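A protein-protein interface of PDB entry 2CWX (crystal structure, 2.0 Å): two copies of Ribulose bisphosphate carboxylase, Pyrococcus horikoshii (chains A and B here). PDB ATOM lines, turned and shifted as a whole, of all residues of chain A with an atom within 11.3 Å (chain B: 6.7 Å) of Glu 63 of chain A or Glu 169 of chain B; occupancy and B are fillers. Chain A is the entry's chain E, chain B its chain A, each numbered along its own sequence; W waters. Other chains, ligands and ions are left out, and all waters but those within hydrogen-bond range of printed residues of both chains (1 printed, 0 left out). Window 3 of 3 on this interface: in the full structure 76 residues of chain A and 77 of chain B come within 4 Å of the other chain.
Trp 55 of chain A touches none of the printed residues of chain B.
Printed residues of chain B within 4 Å of Trp 59 of chain A: Ile 173 (3.3 Å).
Printed residues of chain B within 4 Å of Lys 60 of chain A: Glu 169 (3.7 Å) and Glu 172 (3.0 Å).
Printed residues of chain B within 4 Å of Pro 62 of chain A: Gly 164, Trp 165 and Glu 169.
Of chain B, only Gly 164 (3.9 Å) and Glu 169 (3.2 Å) come within 4 Å of Glu 63 of chain A.
Of the printed residues of chain B, Met 64 of chain A touches Gly 164 (3.3 Å).
Of the printed residues of chain B, Ala 65 of chain A touches Gly 164 (3.9 Å).
Pro 89 of chain A touches none of the printed residues of chain B.
Printed residues of chain A within 4 Å of Gly 164 of chain B: Pro 62 (3.6 Å), Glu 63 (3.9 Å), Met 64 (3.3 Å) and Ala 65 (3.9 Å).
Trp 165 of chain B touches one residue of chain A.
No residue of chain A comes within 4 Å of Ser 166 of chain B.
Printed residues of chain A within 4 Å of Glu 169 of chain B: Lys 60 (3.7 Å), Pro 62 (3.9 Å) and Glu 63 (3.2 Å).
Glu 172 of chain B touches just one residue of chain A: Lys 60 (3.0 Å).
Printed residues of chain A within 4 Å of Ile 173 of chain B: Trp 59 (3.3 Å).
The nearest residue of chain B that does not touch Glu 63 of chain A is Trp 165 of chain B (5.4 Å).
The nearest residue of chain A that does not touch Glu 169 of chain B is Leu 61 of chain A (4.8 Å).
Of the 11 printed residues of chain B, 5 touch a printed residue of chain A.
Along chain B the printed residues that touch a printed residue of chain A span positions 164 to 173.
Hydrophobic or aromatic side chains of chain A that line the printed part of chain B: Trp 59, Pro 62 and Met 64.
Among the printed residues, Asp or Glu carboxylates within 4 Å of a Lys or Arg side-chain nitrogen of the other chain: Lys 60 of chain A with Glu 172 of chain B.
CD1 of Trp 59 of chain A touches CD1 of Ile 173 of chain B, at 3.3 Å.
CE of Lys 60 of chain A touches CG of Glu 169 of chain B, 3.7 Å away.
O of Gly 164 of chain B touches CB of Pro 62 of chain A, at 3.6 Å.
Pro 62 of chain A touches Trp 165 of chain B.
Glu 169 of chain B touches Pro 62 of chain A (OE1 to CB, 3.9 Å).
O of Gly 164 of chain B touches N of Glu 63 of chain A, at 3.9 Å.
N of Ala 65 of chain A touches CA of Gly 164 of chain B, at 3.9 Å.
The side-chain carboxylate (OE1) of Glu 172 of chain B is in salt-bridge range of the side-chain amino group (NZ) of Lys 60 of chain A, at 3.0 Å.
The side-chain carboxylate (OE2) of Glu 63 of chain A lies close to the side-chain carboxylate (OE2) of Glu 169 of chain B (3.2 Å).
The backbone carbonyl oxygen of Gly 164 of chain B lies within hydrogen-bond range of the backbone NH of Met 64 of chain A (3.3 Å).
No position is printed for both chains.
Of the 10 pairs that touch across the chains among the printed residues, none has its exchanged pair printed and touching as well.
Water W1 lies within hydrogen-bond range of the backbone carbonyl oxygen of Gly 164 of chain B (2.9 Å), the side-chain carboxylate of Glu 169 of chain B (3.1 Å), the backbone NH of Glu 63 of chain A (3.1 Å) and the backbone NH of Met 64 of chain A (3.2 Å).
The side-chain carboxylate (OE2) of Glu 172 of chain B lies close to the side-chain carboxylate (OE1) of Glu 168 of chain B, 2.4 Å away.
SD of Met 64 of chain A lies within hydrogen-bond range of NH1 of Arg 67 of chain A (3.5 Å).
The backbone NH (N) of Ser 166 of chain B sits at hydrogen-bond distance from the side-chain carboxylate (OE1) of Glu 169 of chain B (3.0 Å).
O of Met 64 of chain A sits at hydrogen-bond distance from OG of Ser 68 of chain A, 2.9 Å away.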
ATOM      1  N   ILE A  52      -0.591   6.848  12.421  1.00  0.00           N
ATOM      2  CA  ILE A  52      -1.725   5.979  12.213  1.00  0.00           C
ATOM      3  C   ILE A  52      -1.490   4.524  12.569  1.00  0.00           C
ATOM      4  O   ILE A  52      -2.423   3.722  12.520  1.00  0.00           O
ATOM      5  CB  ILE A  52      -2.193   6.076  10.761  1.00  0.00           C
ATOM      6  CG1 ILE A  52      -1.094   5.644   9.790  1.00  0.00           C
ATOM      7  CG2 ILE A  52      -2.652   7.518  10.453  1.00  0.00           C
ATOM      8  CD1 ILE A  52      -1.685   5.147   8.503  1.00  0.00           C
ATOM      9  N   TRP A  55      -1.633  -0.122   8.608  1.00  0.00           N
ATOM     10  CA  TRP A  55      -2.512  -1.031   7.819  1.00  0.00           C
ATOM     11  C   TRP A  55      -2.879  -0.774   6.333  1.00  0.00           C
ATOM     12  O   TRP A  55      -3.233   0.341   5.961  1.00  0.00           O
ATOM     13  CB  TRP A  55      -3.815  -1.285   8.550  1.00  0.00           C
ATOM     14  CG  TRP A  55      -3.910  -2.685   9.016  1.00  0.00           C
ATOM     15  CD1 TRP A  55      -2.891  -3.491   9.481  1.00  0.00           C
ATOM     16  CD2 TRP A  55      -5.095  -3.474   9.057  1.00  0.00           C
ATOM     17  NE1 TRP A  55      -3.389  -4.730   9.818  1.00  0.00           N
ATOM     18  CE2 TRP A  55      -4.741  -4.744   9.573  1.00  0.00           C
ATOM     19  CE3 TRP A  55      -6.436  -3.234   8.719  1.00  0.00           C
ATOM     20  CZ2 TRP A  55      -5.675  -5.764   9.743  1.00  0.00           C
ATOM     21  CZ3 TRP A  55      -7.356  -4.239   8.898  1.00  0.00           C
ATOM     22  CH2 TRP A  55      -6.978  -5.488   9.401  1.00  0.00           C
ATOM     23  N   TRP A  59     -10.774  -5.226   5.636  1.00  0.00           N
ATOM     24  CA  TRP A  59     -11.710  -4.553   6.548  1.00  0.00           C
ATOM     25  C   TRP A  59     -11.542  -3.028   6.606  1.00  0.00           C
ATOM     26  O   TRP A  59     -11.152  -2.464   7.630  1.00  0.00           O
ATOM     27  CB  TRP A  59     -11.729  -5.137   7.975  1.00  0.00           C
ATOM     28  CG  TRP A  59     -13.051  -4.809   8.632  1.00  0.00           C
ATOM     29  CD1 TRP A  59     -13.383  -3.669   9.328  1.00  0.00           C
ATOM     30  CD2 TRP A  59     -14.245  -5.592   8.559  1.00  0.00           C
ATOM     31  NE1 TRP A  59     -14.701  -3.720   9.721  1.00  0.00           N
ATOM     32  CE2 TRP A  59     -15.255  -4.891   9.266  1.00  0.00           C
ATOM     33  CE3 TRP A  59     -14.566  -6.840   7.980  1.00  0.00           C
ATOM     34  CZ2 TRP A  59     -16.558  -5.394   9.409  1.00  0.00           C
ATOM     35  CZ3 TRP A  59     -15.859  -7.342   8.124  1.00  0.00           C
ATOM     36  CH2 TRP A  59     -16.839  -6.618   8.831  1.00  0.00           C
ATOM     37  N   LYS A  60     -11.868  -2.384   5.492  1.00  0.00           N
ATOM     38  CA  LYS A  60     -11.980  -0.927   5.390  1.00  0.00           C
ATOM     39  C   LYS A  60     -10.855  -0.119   6.066  1.00  0.00           C
ATOM     40  O   LYS A  60     -10.775  -0.012   7.295  1.00  0.00           O
ATOM     41  CB  LYS A  60     -13.369  -0.456   5.881  1.00  0.00           C
ATOM     42  CG  LYS A  60     -14.134   0.442   4.864  1.00  0.00           C
ATOM     43  CD  LYS A  60     -15.655   0.535   5.151  1.00  0.00           C
ATOM     44  CE  LYS A  60     -16.026   1.754   6.021  1.00  0.00           C
ATOM     45  NZ  LYS A  60     -17.506   1.867   6.284  1.00  0.00           N
ATOM     46  N   LEU A  61      -9.988   0.433   5.227  1.00  0.00           N
ATOM     47  CA  LEU A  61      -9.103   1.521   5.611  1.00  0.00           C
ATOM     48  C   LEU A  61      -9.999   2.728   5.954  1.00  0.00           C
ATOM     49  O   LEU A  61     -10.893   3.051   5.169  1.00  0.00           O
ATOM     50  CB  LEU A  61      -8.182   1.827   4.431  1.00  0.00           C
ATOM     51  CG  LEU A  61      -7.115   2.917   4.476  1.00  0.00           C
ATOM     52  CD1 LEU A  61      -7.745   4.273   4.579  1.00  0.00           C
ATOM     53  CD2 LEU A  61      -6.112   2.678   5.598  1.00  0.00           C
ATOM     54  N   PRO A  62      -9.808   3.373   7.112  1.00  0.00           N
ATOM     55  CA  PRO A  62     -10.633   4.530   7.473  1.00  0.00           C
ATOM     56  C   PRO A  62     -10.299   5.752   6.637  1.00  0.00           C
ATOM     57  O   PRO A  62      -9.171   5.930   6.164  1.00  0.00           O
ATOM     58  CB  PRO A  62     -10.297   4.775   8.945  1.00  0.00           C
ATOM     59  CG  PRO A  62      -9.438   3.661   9.367  1.00  0.00           C
ATOM     60  CD  PRO A  62      -8.817   3.073   8.152  1.00  0.00           C
ATOM     61  N   GLU A  63     -11.292   6.613   6.463  1.00  0.00           N
ATOM     62  CA  GLU A  63     -11.225   7.626   5.396  1.00  0.00           C
ATOM     63  C   GLU A  63     -10.113   8.666   5.610  1.00  0.00           C
ATOM     64  O   GLU A  63      -9.498   9.096   4.654  1.00  0.00           O
ATOM     65  CB  GLU A  63     -12.599   8.303   5.179  1.00  0.00           C
ATOM     66  CG  GLU A  63     -13.095   8.293   3.730  1.00  0.00           C
ATOM     67  CD  GLU A  63     -13.203   6.897   3.127  1.00  0.00           C
ATOM     68  OE1 GLU A  63     -12.899   6.749   1.917  1.00  0.00           O
ATOM     69  OE2 GLU A  63     -13.595   5.952   3.859  1.00  0.00           O
ATOM     70  N   MET A  64      -9.839   9.019   6.863  1.00  0.00           N
ATOM     71  CA  MET A  64      -8.859  10.041   7.188  1.00  0.00           C
ATOM     72  C   MET A  64      -7.477   9.466   7.538  1.00  0.00           C
ATOM     73  O   MET A  64      -6.560  10.220   7.786  1.00  0.00           O
ATOM     74  CB  MET A  64      -9.370  10.892   8.348  1.00  0.00           C
ATOM     75  CG  MET A  64     -10.531  11.776   7.971  1.00  0.00           C
ATOM     76  SD  MET A  64     -10.130  13.008   6.669  1.00  0.00           S
ATOM     77  CE  MET A  64      -8.848  13.908   7.631  1.00  0.00           C
ATOM     78  N   ALA A  65      -7.339   8.146   7.568  1.00  0.00           N
ATOM     79  CA  ALA A  65      -6.043   7.514   7.872  1.00  0.00           C
ATOM     80  C   ALA A  65      -4.971   7.922   6.874  1.00  0.00           C
ATOM     81  O   ALA A  65      -3.869   8.347   7.260  1.00  0.00           O
ATOM     82  CB  ALA A  65      -6.173   5.978   7.897  1.00  0.00           C
ATOM     83  N   LYS A  66      -5.302   7.822   5.589  1.00  0.00           N
ATOM     84  CA  LYS A  66      -4.324   8.099   4.541  1.00  0.00           C
ATOM     85  C   LYS A  66      -3.825   9.543   4.671  1.00  0.00           C
ATOM     86  O   LYS A  66      -2.626   9.796   4.611  1.00  0.00           O
ATOM     87  CB  LYS A  66      -4.919   7.822   3.141  1.00  0.00           C
ATOM     88  CG  LYS A  66      -3.877   7.861   2.003  1.00  0.00           C
ATOM     89  CD  LYS A  66      -4.253   6.945   0.794  1.00  0.00           C
ATOM     90  CE  LYS A  66      -3.789   7.547  -0.559  1.00  0.00           C
ATOM     91  NZ  LYS A  66      -3.565   6.506  -1.628  1.00  0.00           N
ATOM     92  N   ARG A  67      -4.733  10.477   4.935  1.00  0.00           N
ATOM     93  CA  ARG A  67      -4.347  11.887   5.051  1.00  0.00           C
ATOM     94  C   ARG A  67      -3.674  12.240   6.364  1.00  0.00           C
ATOM     95  O   ARG A  67      -3.220  13.362   6.528  1.00  0.00           O
ATOM     96  CB  ARG A  67      -5.560  12.798   4.911  1.00  0.00           C
ATOM     97  CG  ARG A  67      -6.087  12.882   3.519  1.00  0.00           C
ATOM     98  CD  ARG A  67      -7.498  13.457   3.456  1.00  0.00           C
ATOM     99  NE  ARG A  67      -7.591  14.777   4.102  1.00  0.00           N
ATOM    100  CZ  ARG A  67      -8.730  15.457   4.248  1.00  0.00           C
ATOM    101  NH1 ARG A  67      -9.873  14.957   3.801  1.00  0.00           N
ATOM    102  NH2 ARG A  67      -8.721  16.643   4.834  1.00  0.00           N
ATOM    103  N   SER A  68      -3.665  11.321   7.319  1.00  0.00           N
ATOM    104  CA  SER A  68      -3.068  11.556   8.609  1.00  0.00           C
ATOM    105  C   SER A  68      -1.692  10.871   8.770  1.00  0.00           C
ATOM    106  O   SER A  68      -1.117  10.933   9.839  1.00  0.00           O
ATOM    107  CB  SER A  68      -4.033  11.070   9.708  1.00  0.00           C
ATOM    108  OG  SER A  68      -5.236  11.857   9.726  1.00  0.00           O
ATOM    109  N   MET A  69      -1.156  10.250   7.729  1.00  0.00           N
ATOM    110  CA  MET A  69       0.160   9.626   7.833  1.00  0.00           C
ATOM    111  C   MET A  69       1.281  10.639   8.078  1.00  0.00           C
ATOM    112  O   MET A  69       1.444  11.580   7.321  1.00  0.00           O
ATOM    113  CB  MET A  69       0.504   8.859   6.563  1.00  0.00           C
ATOM    114  CG  MET A  69      -0.175   7.533   6.499  1.00  0.00           C
ATOM    115  SD  MET A  69       0.274   6.579   4.996  1.00  0.00           S
ATOM    116  CE  MET A  69       2.033   6.752   4.987  1.00  0.00           C
ATOM    117  N   PRO A  89       0.679  15.814   9.638  1.00  0.00           N
ATOM    118  CA  PRO A  89      -0.490  16.590   9.260  1.00  0.00           C
ATOM    119  C   PRO A  89      -1.344  16.897  10.487  1.00  0.00           C
ATOM    120  O   PRO A  89      -1.401  16.142  11.434  1.00  0.00           O
ATOM    121  CB  PRO A  89      -1.254  15.656   8.348  1.00  0.00           C
ATOM    122  CG  PRO A  89      -0.215  14.646   7.908  1.00  0.00           C
ATOM    123  CD  PRO A  89       0.583  14.418   9.151  1.00  0.00           C
ATOM    124  N   THR A  91      -4.459  16.951  10.897  1.00  0.00           N
ATOM    125  CA  THR A  91      -5.535  15.984  11.106  1.00  0.00           C
ATOM    126  C   THR A  91      -5.245  14.967  12.187  1.00  0.00           C
ATOM    127  O   THR A  91      -6.175  14.317  12.639  1.00  0.00           O
ATOM    128  CB  THR A  91      -5.803  15.200   9.810  1.00  0.00           C
ATOM    129  OG1 THR A  91      -4.550  14.923   9.194  1.00  0.00           O
ATOM    130  CG2 THR A  91      -6.501  16.069   8.822  1.00  0.00           C
ATOM    131  N   LEU A  92      -3.984  14.850  12.609  1.00  0.00           N
ATOM    132  CA  LEU A  92      -3.590  13.924  13.674  1.00  0.00           C
ATOM    133  C   LEU A  92      -3.875  14.447  15.062  1.00  0.00           C
ATOM    134  O   LEU A  92      -3.777  13.709  16.030  1.00  0.00           O
ATOM    135  CB  LEU A  92      -2.086  13.599  13.585  1.00  0.00           C
ATOM    136  CG  LEU A  92      -1.723  12.577  12.501  1.00  0.00           C
ATOM    137  CD1 LEU A  92      -0.221  12.554  12.347  1.00  0.00           C
ATOM    138  CD2 LEU A  92      -2.252  11.207  12.900  1.00  0.00           C
ATOM    139  N   GLY B 164      -8.094   7.876  12.455  1.00  0.00           N
ATOM    140  CA  GLY B 164      -8.679   8.317  11.213  1.00  0.00           C
ATOM    141  C   GLY B 164     -10.129   7.924  10.994  1.00  0.00           C
ATOM    142  O   GLY B 164     -10.694   8.206   9.959  1.00  0.00           O
ATOM    143  N   TRP B 165     -10.726   7.252  11.958  1.00  0.00           N
ATOM    144  CA  TRP B 165     -12.090   6.747  11.819  1.00  0.00           C
ATOM    145  C   TRP B 165     -13.132   7.822  12.027  1.00  0.00           C
ATOM    146  O   TRP B 165     -13.009   8.614  12.954  1.00  0.00           O
ATOM    147  CB  TRP B 165     -12.359   5.716  12.888  1.00  0.00           C
ATOM    148  CG  TRP B 165     -11.362   4.647  12.968  1.00  0.00           C
ATOM    149  CD1 TRP B 165     -10.228   4.639  13.721  1.00  0.00           C
ATOM    150  CD2 TRP B 165     -11.406   3.406  12.293  1.00  0.00           C
ATOM    151  NE1 TRP B 165      -9.563   3.449  13.544  1.00  0.00           N
ATOM    152  CE2 TRP B 165     -10.264   2.678  12.672  1.00  0.00           C
ATOM    153  CE3 TRP B 165     -12.308   2.819  11.414  1.00  0.00           C
ATOM    154  CZ2 TRP B 165      -9.997   1.407  12.200  1.00  0.00           C
ATOM    155  CZ3 TRP B 165     -12.038   1.555  10.933  1.00  0.00           C
ATOM    156  CH2 TRP B 165     -10.886   0.865  11.324  1.00  0.00           C
ATOM    157  N   SER B 166     -14.178   7.797  11.196  1.00  0.00           N
ATOM    158  CA  SER B 166     -15.433   8.501  11.486  1.00  0.00           C
ATOM    159  C   SER B 166     -16.134   7.787  12.653  1.00  0.00           C
ATOM    160  O   SER B 166     -15.808   6.656  12.963  1.00  0.00           O
ATOM    161  CB  SER B 166     -16.330   8.532  10.246  1.00  0.00           C
ATOM    162  OG  SER B 166     -16.837   7.220   9.945  1.00  0.00           O
ATOM    163  N   VAL B 167     -17.095   8.427  13.294  1.00  0.00           N
ATOM    164  CA  VAL B 167     -17.885   7.794  14.355  1.00  0.00           C
ATOM    165  C   VAL B 167     -18.615   6.576  13.804  1.00  0.00           C
ATOM    166  O   VAL B 167     -18.668   5.529  14.444  1.00  0.00           O
ATOM    167  CB  VAL B 167     -18.872   8.814  14.977  1.00  0.00           C
ATOM    168  CG1 VAL B 167     -19.888   8.143  15.923  1.00  0.00           C
ATOM    169  CG2 VAL B 167     -18.073   9.899  15.744  1.00  0.00           C
ATOM    170  N   GLU B 168     -19.152   6.687  12.591  1.00  0.00           N
ATOM    171  CA  GLU B 168     -19.873   5.555  11.997  1.00  0.00           C
ATOM    172  C   GLU B 168     -18.998   4.348  11.700  1.00  0.00           C
ATOM    173  O   GLU B 168     -19.396   3.219  11.978  1.00  0.00           O
ATOM    174  CB  GLU B 168     -20.588   5.968  10.727  1.00  0.00           C
ATOM    175  CG  GLU B 168     -22.034   5.547  10.744  1.00  0.00           C
ATOM    176  CD  GLU B 168     -22.215   4.048  10.538  1.00  0.00           C
ATOM    177  OE1 GLU B 168     -21.496   3.502   9.661  1.00  0.00           O
ATOM    178  OE2 GLU B 168     -23.070   3.437  11.244  1.00  0.00           O
ATOM    179  N   GLU B 169     -17.817   4.590  11.135  1.00  0.00           N
ATOM    180  CA  GLU B 169     -16.844   3.521  10.898  1.00  0.00           C
ATOM    181  C   GLU B 169     -16.410   2.875  12.220  1.00  0.00           C
ATOM    182  O   GLU B 169     -16.337   1.658  12.332  1.00  0.00           O
ATOM    183  CB  GLU B 169     -15.621   4.039  10.148  1.00  0.00           C
ATOM    184  CG  GLU B 169     -15.844   4.393   8.671  1.00  0.00           C
ATOM    185  CD  GLU B 169     -14.785   5.362   8.079  1.00  0.00           C
ATOM    186  OE1 GLU B 169     -14.015   6.058   8.815  1.00  0.00           O
ATOM    187  OE2 GLU B 169     -14.709   5.429   6.837  1.00  0.00           O
ATOM    188  N   TYR B 170     -16.159   3.695  13.231  1.00  0.00           N
ATOM    189  CA  TYR B 170     -15.742   3.195  14.531  1.00  0.00           C
ATOM    190  C   TYR B 170     -16.832   2.331  15.161  1.00  0.00           C
ATOM    191  O   TYR B 170     -16.545   1.298  15.743  1.00  0.00           O
ATOM    192  CB  TYR B 170     -15.425   4.343  15.455  1.00  0.00           C
ATOM    193  CG  TYR B 170     -14.348   4.088  16.474  1.00  0.00           C
ATOM    194  CD1 TYR B 170     -13.013   3.957  16.085  1.00  0.00           C
ATOM    195  CD2 TYR B 170     -14.637   4.051  17.822  1.00  0.00           C
ATOM    196  CE1 TYR B 170     -12.023   3.768  17.000  1.00  0.00           C
ATOM    197  CE2 TYR B 170     -13.659   3.865  18.740  1.00  0.00           C
ATOM    198  CZ  TYR B 170     -12.337   3.705  18.331  1.00  0.00           C
ATOM    199  OH  TYR B 170     -11.286   3.535  19.250  1.00  0.00           O
ATOM    200  N   ALA B 171     -18.081   2.796  15.061  1.00  0.00           N
ATOM    201  CA  ALA B 171     -19.242   2.041  15.529  1.00  0.00           C
ATOM    202  C   ALA B 171     -19.303   0.657  14.880  1.00  0.00           C
ATOM    203  O   ALA B 171     -19.630  -0.302  15.551  1.00  0.00           O
ATOM    204  CB  ALA B 171     -20.554   2.821  15.265  1.00  0.00           C
ATOM    205  N   GLU B 172     -19.011   0.575  13.583  1.00  0.00           N
ATOM    206  CA  GLU B 172     -19.089  -0.691  12.843  1.00  0.00           C
ATOM    207  C   GLU B 172     -17.997  -1.644  13.297  1.00  0.00           C
ATOM    208  O   GLU B 172     -18.288  -2.784  13.542  1.00  0.00           O
ATOM    209  CB  GLU B 172     -18.969  -0.462  11.329  1.00  0.00           C
ATOM    210  CG  GLU B 172     -20.183   0.243  10.747  1.00  0.00           C
ATOM    211  CD  GLU B 172     -20.027   0.748   9.293  1.00  0.00           C
ATOM    212  OE1 GLU B 172     -18.933   0.638   8.662  1.00  0.00           O
ATOM    213  OE2 GLU B 172     -21.030   1.304   8.782  1.00  0.00           O
ATOM    214  N   ILE B 173     -16.751  -1.174  13.438  1.00  0.00           N
ATOM    215  CA  ILE B 173     -15.661  -2.010  13.993  1.00  0.00           C
ATOM    216  C   ILE B 173     -16.019  -2.460  15.420  1.00  0.00           C
ATOM    217  O   ILE B 173     -15.920  -3.637  15.750  1.00  0.00           O
ATOM    218  CB  ILE B 173     -14.287  -1.302  14.001  1.00  0.00           C
ATOM    219  CG1 ILE B 173     -14.002  -0.602  12.679  1.00  0.00           C
ATOM    220  CG2 ILE B 173     -13.140  -2.290  14.265  1.00  0.00           C
ATOM    221  CD1 ILE B 173     -13.226  -1.425  11.690  1.00  0.00           C
ATOM    222  N   ALA B 174     -16.455  -1.535  16.264  1.00  0.00           N
ATOM    223  CA  ALA B 174     -16.836  -1.893  17.630  1.00  0.00           C
ATOM    224  C   ALA B 174     -17.872  -2.988  17.631  1.00  0.00           C
ATOM    225  O   ALA B 174     -17.732  -3.981  18.337  1.00  0.00           O
ATOM    226  CB  ALA B 174     -17.364  -0.696  18.393  1.00  0.00           C
HETATM  227  O   HOH W   1     -12.813   8.775   8.084  1.00  0.00           O
